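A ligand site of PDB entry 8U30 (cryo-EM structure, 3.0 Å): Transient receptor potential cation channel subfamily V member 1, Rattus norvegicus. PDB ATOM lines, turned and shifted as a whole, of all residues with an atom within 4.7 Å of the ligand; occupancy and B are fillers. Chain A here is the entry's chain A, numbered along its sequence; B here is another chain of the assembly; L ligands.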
ATOM      1  N   SER A 402      31.028  16.425  30.037  1.00  0.00           N
ATOM      2  CA  SER A 402      32.045  17.437  30.274  1.00  0.00           C
ATOM      3  C   SER A 402      32.300  18.220  28.994  1.00  0.00           C
ATOM      4  O   SER A 402      32.359  17.658  27.899  1.00  0.00           O
ATOM      5  CB  SER A 402      33.344  16.800  30.763  1.00  0.00           C
ATOM      6  OG  SER A 402      33.770  15.778  29.889  1.00  0.00           O
ATOM      7  N   ARG A 409      39.034  13.861  28.084  1.00  0.00           N
ATOM      8  CA  ARG A 409      37.673  13.324  28.056  1.00  0.00           C
ATOM      9  C   ARG A 409      37.571  12.080  27.195  1.00  0.00           C
ATOM     10  O   ARG A 409      36.780  11.175  27.492  1.00  0.00           O
ATOM     11  CB  ARG A 409      36.711  14.400  27.568  1.00  0.00           C
ATOM     12  CG  ARG A 409      36.949  14.859  26.143  1.00  0.00           C
ATOM     13  CD  ARG A 409      36.078  16.049  25.812  1.00  0.00           C
ATOM     14  NE  ARG A 409      34.703  15.649  25.519  1.00  0.00           N
ATOM     15  CZ  ARG A 409      33.734  15.592  26.415  1.00  0.00           C
ATOM     16  NH1 ARG A 409      33.934  15.885  27.687  1.00  0.00           N
ATOM     17  NH2 ARG A 409      32.509  15.233  26.026  1.00  0.00           N
ATOM     18  N   HIS A 410      38.354  11.992  26.111  1.00  0.00           N
ATOM     19  CA  HIS A 410      38.287  10.830  25.241  1.00  0.00           C
ATOM     20  C   HIS A 410      38.899   9.604  25.895  1.00  0.00           C
ATOM     21  O   HIS A 410      38.311   8.507  25.852  1.00  0.00           O
ATOM     22  CB  HIS A 410      39.004  11.119  23.916  1.00  0.00           C
ATOM     23  CG  HIS A 410      38.406  12.249  23.151  1.00  0.00           C
ATOM     24  ND1 HIS A 410      37.055  12.528  23.154  1.00  0.00           N
ATOM     25  CD2 HIS A 410      38.973  13.168  22.338  1.00  0.00           C
ATOM     26  CE1 HIS A 410      36.821  13.582  22.390  1.00  0.00           C
ATOM     27  NE2 HIS A 410      37.966  13.991  21.881  1.00  0.00           N
ATOM     28  N   VAL A 508      31.545  23.781  18.493  1.00  0.00           N
ATOM     29  CA  VAL A 508      32.613  22.813  18.693  1.00  0.00           C
ATOM     30  C   VAL A 508      32.094  21.444  19.112  1.00  0.00           C
ATOM     31  O   VAL A 508      32.777  20.439  18.858  1.00  0.00           O
ATOM     32  CB  VAL A 508      33.640  23.325  19.715  1.00  0.00           C
ATOM     33  CG1 VAL A 508      34.893  22.460  19.686  1.00  0.00           C
ATOM     34  CG2 VAL A 508      33.987  24.778  19.444  1.00  0.00           C
ATOM     35  N   ASP A 509      30.931  21.357  19.751  1.00  0.00           N
ATOM     36  CA  ASP A 509      30.355  20.089  20.170  1.00  0.00           C
ATOM     37  C   ASP A 509      28.865  20.093  19.865  1.00  0.00           C
ATOM     38  O   ASP A 509      28.246  21.144  19.698  1.00  0.00           O
ATOM     39  CB  ASP A 509      30.566  19.835  21.675  1.00  0.00           C
ATOM     40  CG  ASP A 509      32.031  19.734  22.041  1.00  0.00           C
ATOM     41  OD1 ASP A 509      32.836  19.332  21.177  1.00  0.00           O
ATOM     42  OD2 ASP A 509      32.371  20.041  23.200  1.00  0.00           O
ATOM     43  N   SER A 510      28.258  18.912  19.871  1.00  0.00           N
ATOM     44  CA  SER A 510      26.824  18.739  19.538  1.00  0.00           C
ATOM     45  C   SER A 510      26.566  19.151  18.087  1.00  0.00           C
ATOM     46  O   SER A 510      25.654  19.950  17.864  1.00  0.00           O
ATOM     47  CB  SER A 510      25.933  19.474  20.523  1.00  0.00           C
ATOM     48  OG  SER A 510      25.809  20.862  20.241  1.00  0.00           O
ATOM     49  N   TYR A 511      27.314  18.618  17.114  1.00  0.00           N
ATOM     50  CA  TYR A 511      27.016  18.865  15.710  1.00  0.00           C
ATOM     51  C   TYR A 511      25.722  18.186  15.294  1.00  0.00           C
ATOM     52  O   TYR A 511      24.927  18.773  14.542  1.00  0.00           O
ATOM     53  CB  TYR A 511      28.177  18.380  14.836  1.00  0.00           C
ATOM     54  CG  TYR A 511      29.440  19.194  14.999  1.00  0.00           C
ATOM     55  CD1 TYR A 511      29.499  20.502  14.551  1.00  0.00           C
ATOM     56  CD2 TYR A 511      30.565  18.652  15.600  1.00  0.00           C
ATOM     57  CE1 TYR A 511      30.651  21.248  14.707  1.00  0.00           C
ATOM     58  CE2 TYR A 511      31.716  19.388  15.753  1.00  0.00           C
ATOM     59  CZ  TYR A 511      31.752  20.688  15.306  1.00  0.00           C
ATOM     60  OH  TYR A 511      32.907  21.438  15.449  1.00  0.00           O
ATOM     61  N   SER A 512      25.493  16.958  15.756  1.00  0.00           N
ATOM     62  CA  SER A 512      24.275  16.241  15.373  1.00  0.00           C
ATOM     63  C   SER A 512      23.036  16.983  15.840  1.00  0.00           C
ATOM     64  O   SER A 512      22.042  17.099  15.102  1.00  0.00           O
ATOM     65  CB  SER A 512      24.303  14.831  15.966  1.00  0.00           C
ATOM     66  OG  SER A 512      25.460  14.133  15.563  1.00  0.00           O
ATOM     67  N   LEU A 515      22.411  20.033  13.694  1.00  0.00           N
ATOM     68  CA  LEU A 515      21.968  19.644  12.348  1.00  0.00           C
ATOM     69  C   LEU A 515      20.500  19.226  12.353  1.00  0.00           C
ATOM     70  O   LEU A 515      19.729  19.625  11.475  1.00  0.00           O
ATOM     71  CB  LEU A 515      22.853  18.525  11.811  1.00  0.00           C
ATOM     72  CG  LEU A 515      24.258  18.936  11.408  1.00  0.00           C
ATOM     73  CD1 LEU A 515      25.083  17.713  11.086  1.00  0.00           C
ATOM     74  CD2 LEU A 515      24.243  19.879  10.232  1.00  0.00           C
ATOM     75  N   THR A 550      21.001  13.344   4.687  1.00  0.00           N
ATOM     76  CA  THR A 550      22.370  13.342   5.187  1.00  0.00           C
ATOM     77  C   THR A 550      22.436  13.019   6.670  1.00  0.00           C
ATOM     78  O   THR A 550      23.344  12.287   7.103  1.00  0.00           O
ATOM     79  CB  THR A 550      23.047  14.683   4.915  1.00  0.00           C
ATOM     80  OG1 THR A 550      22.289  15.731   5.500  1.00  0.00           O
ATOM     81  CG2 THR A 550      23.193  14.920   3.424  1.00  0.00           C
ATOM     82  N   ASN A 551      21.505  13.526   7.472  1.00  0.00           N
ATOM     83  CA  ASN A 551      21.466  13.231   8.900  1.00  0.00           C
ATOM     84  C   ASN A 551      21.217  11.756   9.169  1.00  0.00           C
ATOM     85  O   ASN A 551      21.492  11.291  10.276  1.00  0.00           O
ATOM     86  CB  ASN A 551      20.396  14.053   9.610  1.00  0.00           C
ATOM     87  CG  ASN A 551      20.767  15.505   9.749  1.00  0.00           C
ATOM     88  OD1 ASN A 551      21.934  15.840   9.951  1.00  0.00           O
ATOM     89  ND2 ASN A 551      19.779  16.373   9.685  1.00  0.00           N
ATOM     90  N   LEU A 553      23.057   9.694   8.524  1.00  0.00           N
ATOM     91  CA  LEU A 553      24.383   9.180   8.856  1.00  0.00           C
ATOM     92  C   LEU A 553      24.647   9.172  10.358  1.00  0.00           C
ATOM     93  O   LEU A 553      25.644   8.586  10.792  1.00  0.00           O
ATOM     94  CB  LEU A 553      25.439  10.025   8.132  1.00  0.00           C
ATOM     95  CG  LEU A 553      26.904   9.640   8.276  1.00  0.00           C
ATOM     96  CD1 LEU A 553      27.147   8.267   7.696  1.00  0.00           C
ATOM     97  CD2 LEU A 553      27.795  10.669   7.600  1.00  0.00           C
ATOM     98  N   TYR A 554      23.797   9.819  11.151  1.00  0.00           N
ATOM     99  CA  TYR A 554      24.000   9.832  12.603  1.00  0.00           C
ATOM    100  C   TYR A 554      23.922   8.436  13.189  1.00  0.00           C
ATOM    101  O   TYR A 554      24.707   8.086  14.075  1.00  0.00           O
ATOM    102  CB  TYR A 554      22.957  10.739  13.258  1.00  0.00           C
ATOM    103  CG  TYR A 554      22.713  10.457  14.727  1.00  0.00           C
ATOM    104  CD1 TYR A 554      23.455  11.098  15.710  1.00  0.00           C
ATOM    105  CD2 TYR A 554      21.742   9.554  15.133  1.00  0.00           C
ATOM    106  CE1 TYR A 554      23.239  10.838  17.049  1.00  0.00           C
ATOM    107  CE2 TYR A 554      21.525   9.284  16.470  1.00  0.00           C
ATOM    108  CZ  TYR A 554      22.266   9.935  17.417  1.00  0.00           C
ATOM    109  OH  TYR A 554      22.044   9.678  18.749  1.00  0.00           O
ATOM    110  N   ARG A 557      26.664   5.244  14.161  1.00  0.00           N
ATOM    111  CA  ARG A 557      27.142   4.758  15.447  1.00  0.00           C
ATOM    112  C   ARG A 557      26.253   3.616  15.925  1.00  0.00           C
ATOM    113  O   ARG A 557      25.081   3.517  15.552  1.00  0.00           O
ATOM    114  CB  ARG A 557      27.186   5.875  16.487  1.00  0.00           C
ATOM    115  CG  ARG A 557      25.820   6.400  16.891  1.00  0.00           C
ATOM    116  CD  ARG A 557      25.957   7.694  17.667  1.00  0.00           C
ATOM    117  NE  ARG A 557      26.385   8.796  16.816  1.00  0.00           N
ATOM    118  CZ  ARG A 557      26.562  10.039  17.231  1.00  0.00           C
ATOM    119  NH1 ARG A 557      26.353  10.385  18.489  1.00  0.00           N
ATOM    120  NH2 ARG A 557      26.952  10.974  16.360  1.00  0.00           N
ATOM    121  N   ILE A 569      35.193  11.047   8.725  1.00  0.00           N
ATOM    122  CA  ILE A 569      34.590  12.066   7.872  1.00  0.00           C
ATOM    123  C   ILE A 569      34.498  13.388   8.607  1.00  0.00           C
ATOM    124  O   ILE A 569      34.766  14.461   8.047  1.00  0.00           O
ATOM    125  CB  ILE A 569      33.197  11.609   7.377  1.00  0.00           C
ATOM    126  CG1 ILE A 569      33.353  10.512   6.326  1.00  0.00           C
ATOM    127  CG2 ILE A 569      32.412  12.788   6.821  1.00  0.00           C
ATOM    128  CD1 ILE A 569      32.063   9.818   5.966  1.00  0.00           C
ATOM    129  N   GLU A 570      34.081  13.349   9.878  1.00  0.00           N
ATOM    130  CA  GLU A 570      33.897  14.570  10.646  1.00  0.00           C
ATOM    131  C   GLU A 570      35.217  15.309  10.830  1.00  0.00           C
ATOM    132  O   GLU A 570      35.312  16.522  10.593  1.00  0.00           O
ATOM    133  CB  GLU A 570      33.238  14.199  11.975  1.00  0.00           C
ATOM    134  CG  GLU A 570      32.730  15.336  12.849  1.00  0.00           C
ATOM    135  CD  GLU A 570      33.769  15.974  13.712  1.00  0.00           C
ATOM    136  OE1 GLU A 570      34.736  15.291  14.094  1.00  0.00           O
ATOM    137  OE2 GLU A 570      33.605  17.158  14.074  1.00  0.00           O
ATOM    138  N   LYS A 571      36.273  14.579  11.192  1.00  0.00           N
ATOM    139  CA  LYS A 571      37.597  15.199  11.317  1.00  0.00           C
ATOM    140  C   LYS A 571      38.073  15.797   9.998  1.00  0.00           C
ATOM    141  O   LYS A 571      38.608  16.910   9.969  1.00  0.00           O
ATOM    142  CB  LYS A 571      38.632  14.159  11.789  1.00  0.00           C
ATOM    143  CG  LYS A 571      38.299  13.362  13.045  1.00  0.00           C
ATOM    144  CD  LYS A 571      37.562  14.173  14.099  1.00  0.00           C
ATOM    145  CE  LYS A 571      38.483  15.153  14.799  1.00  0.00           C
ATOM    146  NZ  LYS A 571      37.959  15.546  16.140  1.00  0.00           N
ATOM    147  N   ILE A 573      36.347  16.836   7.376  1.00  0.00           N
ATOM    148  CA  ILE A 573      35.589  18.043   7.083  1.00  0.00           C
ATOM    149  C   ILE A 573      36.122  19.200   7.916  1.00  0.00           C
ATOM    150  O   ILE A 573      36.297  20.313   7.402  1.00  0.00           O
ATOM    151  CB  ILE A 573      34.088  17.820   7.340  1.00  0.00           C
ATOM    152  CG1 ILE A 573      33.485  16.946   6.234  1.00  0.00           C
ATOM    153  CG2 ILE A 573      33.360  19.163   7.413  1.00  0.00           C
ATOM    154  CD1 ILE A 573      32.057  16.519   6.517  1.00  0.00           C
ATOM    155  N   ILE A 673      36.876   8.528  20.053  1.00  0.00           N
ATOM    156  CA  ILE A 673      35.761   9.446  19.869  1.00  0.00           C
ATOM    157  C   ILE A 673      34.478   8.669  19.578  1.00  0.00           C
ATOM    158  O   ILE A 673      33.384   9.041  20.036  1.00  0.00           O
ATOM    159  CB  ILE A 673      36.066  10.459  18.752  1.00  0.00           C
ATOM    160  CG1 ILE A 673      37.228  11.359  19.179  1.00  0.00           C
ATOM    161  CG2 ILE A 673      34.847  11.297  18.447  1.00  0.00           C
ATOM    162  CD1 ILE A 673      37.862  12.107  18.045  1.00  0.00           C
ATOM    163  N   GLN A 677      31.025   8.733  21.733  1.00  0.00           N
ATOM    164  CA  GLN A 677      29.743   8.987  21.039  1.00  0.00           C
ATOM    165  C   GLN A 677      28.731   7.913  21.438  1.00  0.00           C
ATOM    166  O   GLN A 677      27.568   8.273  21.592  1.00  0.00           O
ATOM    167  CB  GLN A 677      29.933   8.983  19.532  1.00  0.00           C
ATOM    168  CG  GLN A 677      30.449  10.289  18.963  1.00  0.00           C
ATOM    169  CD  GLN A 677      30.769  10.187  17.491  1.00  0.00           C
ATOM    170  OE1 GLN A 677      30.601   9.146  16.870  1.00  0.00           O
ATOM    171  NE2 GLN A 677      31.243  11.277  16.927  1.00  0.00           N
ATOM    172  N   ILE A 680      27.673   8.491  25.182  1.00  0.00           N
ATOM    173  CA  ILE A 680      26.672   9.548  25.275  1.00  0.00           C
ATOM    174  C   ILE A 680      25.310   9.027  24.851  1.00  0.00           C
ATOM    175  O   ILE A 680      24.276   9.351  25.454  1.00  0.00           O
ATOM    176  CB  ILE A 680      27.097  10.773  24.433  1.00  0.00           C
ATOM    177  CG1 ILE A 680      28.366  11.389  25.013  1.00  0.00           C
ATOM    178  CG2 ILE A 680      25.979  11.798  24.394  1.00  0.00           C
ATOM    179  CD1 ILE A 680      29.037  12.375  24.095  1.00  0.00           C
ATOM    180  N   LEU B 646      30.618  17.373  -1.313  1.00  0.00           N
ATOM    181  CA  LEU B 646      30.523  16.306  -0.321  1.00  0.00           C
ATOM    182  C   LEU B 646      31.037  14.984  -0.864  1.00  0.00           C
ATOM    183  O   LEU B 646      31.707  14.239  -0.128  1.00  0.00           O
ATOM    184  CB  LEU B 646      29.072  16.165   0.150  1.00  0.00           C
ATOM    185  CG  LEU B 646      28.657  17.087   1.304  1.00  0.00           C
ATOM    186  CD1 LEU B 646      27.165  17.021   1.520  1.00  0.00           C
ATOM    187  CD2 LEU B 646      29.397  16.730   2.572  1.00  0.00           C
HETATM  188  C1  LIG L   1      30.687  14.762  18.775  1.00  0.00           C
HETATM  189  O1  LIG L   1      29.874  13.946  18.002  1.00  0.00           O
HETATM  190  P1  LIG L   1      28.536  14.630  17.327  1.00  0.00           P
HETATM  191  C2  LIG L   1      31.422  15.740  17.859  1.00  0.00           C
HETATM  192  O2  LIG L   1      32.385  15.070  17.102  1.00  0.00           O
HETATM  193  C3  LIG L   1      32.031  16.843  18.706  1.00  0.00           C
HETATM  194  O3  LIG L   1      33.126  17.395  18.040  1.00  0.00           O
HETATM  195  C4  LIG L   1      32.467  16.356  20.087  1.00  0.00           C
HETATM  196  O4  LIG L   1      31.427  16.621  20.986  1.00  0.00           O
HETATM  197  P2  LIG L   1      31.639  16.329  22.592  1.00  0.00           P
HETATM  198  C5  LIG L   1      32.860  14.868  20.081  1.00  0.00           C
HETATM  199  O5  LIG L   1      33.961  14.674  19.241  1.00  0.00           O
HETATM  200  P3  LIG L   1      35.403  15.447  19.477  1.00  0.00           P
HETATM  201  C6  LIG L   1      31.707  13.972  19.598  1.00  0.00           C
HETATM  202  O6  LIG L   1      31.051  13.416  20.688  1.00  0.00           O
HETATM  203  O7  LIG L   1      27.330  13.904  17.647  1.00  0.00           O
HETATM  204  O8  LIG L   1      28.206  15.869  18.014  1.00  0.00           O
HETATM  205  O9  LIG L   1      28.755  14.911  15.720  1.00  0.00           O
HETATM  206  C7  LIG L   1      26.300  13.759  12.122  1.00  0.00           C
HETATM  207  O10 LIG L   1      25.451  13.326  12.817  1.00  0.00           O
HETATM  208  C8  LIG L   1      30.100  16.027  10.785  1.00  0.00           C
HETATM  209  O11 LIG L   1      30.529  15.092  10.200  1.00  0.00           O
HETATM  210  C9  LIG L   1      28.551  13.931  14.745  1.00  0.00           C
HETATM  211  C10 LIG L   1      25.920  14.420  10.802  1.00  0.00           C
HETATM  212  C11 LIG L   1      30.744  17.396  10.574  1.00  0.00           C
HETATM  213  C12 LIG L   1      28.104  14.612  13.456  1.00  0.00           C
HETATM  214  O12 LIG L   1      27.648  13.665  12.513  1.00  0.00           O
HETATM  215  C13 LIG L   1      26.262  13.515   9.617  1.00  0.00           C
HETATM  216  C14 LIG L   1      29.970  18.477  11.312  1.00  0.00           C
HETATM  217  C15 LIG L   1      29.308  15.343  12.892  1.00  0.00           C
HETATM  218  O13 LIG L   1      28.999  15.872  11.640  1.00  0.00           O
HETATM  219  O14 LIG L   1      31.193  15.007  22.998  1.00  0.00           O
HETATM  220  O15 LIG L   1      30.922  17.222  23.493  1.00  0.00           O
HETATM  221  O16 LIG L   1      33.025  16.433  23.040  1.00  0.00           O
HETATM  222  C16 LIG L   1      27.415  14.171   8.855  1.00  0.00           C
HETATM  223  C17 LIG L   1      28.782  18.843  10.434  1.00  0.00           C
HETATM  224  O17 LIG L   1      35.673  16.529  18.542  1.00  0.00           O
HETATM  225  O18 LIG L   1      36.570  14.583  19.292  1.00  0.00           O
HETATM  226  O19 LIG L   1      35.601  16.040  20.795  1.00  0.00           O
HETATM  227  C18 LIG L   1      26.889  15.020   7.713  1.00  0.00           C
HETATM  228  C19 LIG L   1      28.079  20.060  11.027  1.00  0.00           C
HETATM  229  C20 LIG L   1      27.889  16.139   7.456  1.00  0.00           C
HETATM  230  C21 LIG L   1      28.791  21.331  10.574  1.00  0.00           C
HETATM  231  C22 LIG L   1      27.313  17.105   6.446  1.00  0.00           C
HETATM  232  C23 LIG L   1      28.394  21.660   9.144  1.00  0.00           C
HETATM  233  C24 LIG L   1      27.659  18.527   6.891  1.00  0.00           C
HETATM  234  C25 LIG L   1      29.025  22.985   8.756  1.00  0.00           C
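The guanidinium group of Arg 409 lies close to the backbone carbonyl oxygen of Ser 402, 3.1 Å away.
The guanidinium group (NE) of Arg 557 sits at hydrogen-bond distance from the backbone carbonyl oxygen (O) of Tyr 554 (3.3 Å).
The side-chain carboxylate (OE1) of Glu 570 is in salt-bridge range of the side-chain amino group (NZ) of Lys 571, at 3.8 Å.
OD1 of Asp 509 lies close to O4 of the ligand (3.1 Å).
Residues that only touch the ligand: Ile 673, Glu 570, Leu 515, Ser 510, Ile 680, Tyr 554 and Leu 553.
An oxygen (O7) of the ligand is in hydrogen-bond range of the side-chain hydroxyl of Ser 512 (2.8 Å).
NE2 of His 410 sits at hydrogen-bond distance from O18 of the ligand (3.0 Å).
The backbone NH of Tyr 511 is in hydrogen-bond range of an oxygen (O8) of the ligand, at 3.0 Å.
An oxygen (O16) of the ligand is in salt-bridge range of the guanidinium group (NE) of Arg 409 (3.1 Å).
The backbone carbonyl oxygen (O) of Val 508 is in hydrogen-bond range of an oxygen (O3) of the ligand (3.2 Å).
NE2 of Gln 677 is in hydrogen-bond range of O1 of the ligand (3.2 Å).
NH2 of Arg 557 lies within salt-bridge range of O7 of the ligand, 3.2 Å away.
The side-chain amino group (NZ) of Lys 571 is in salt-bridge range of an oxygen (O17) of the ligand (3.5 Å).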
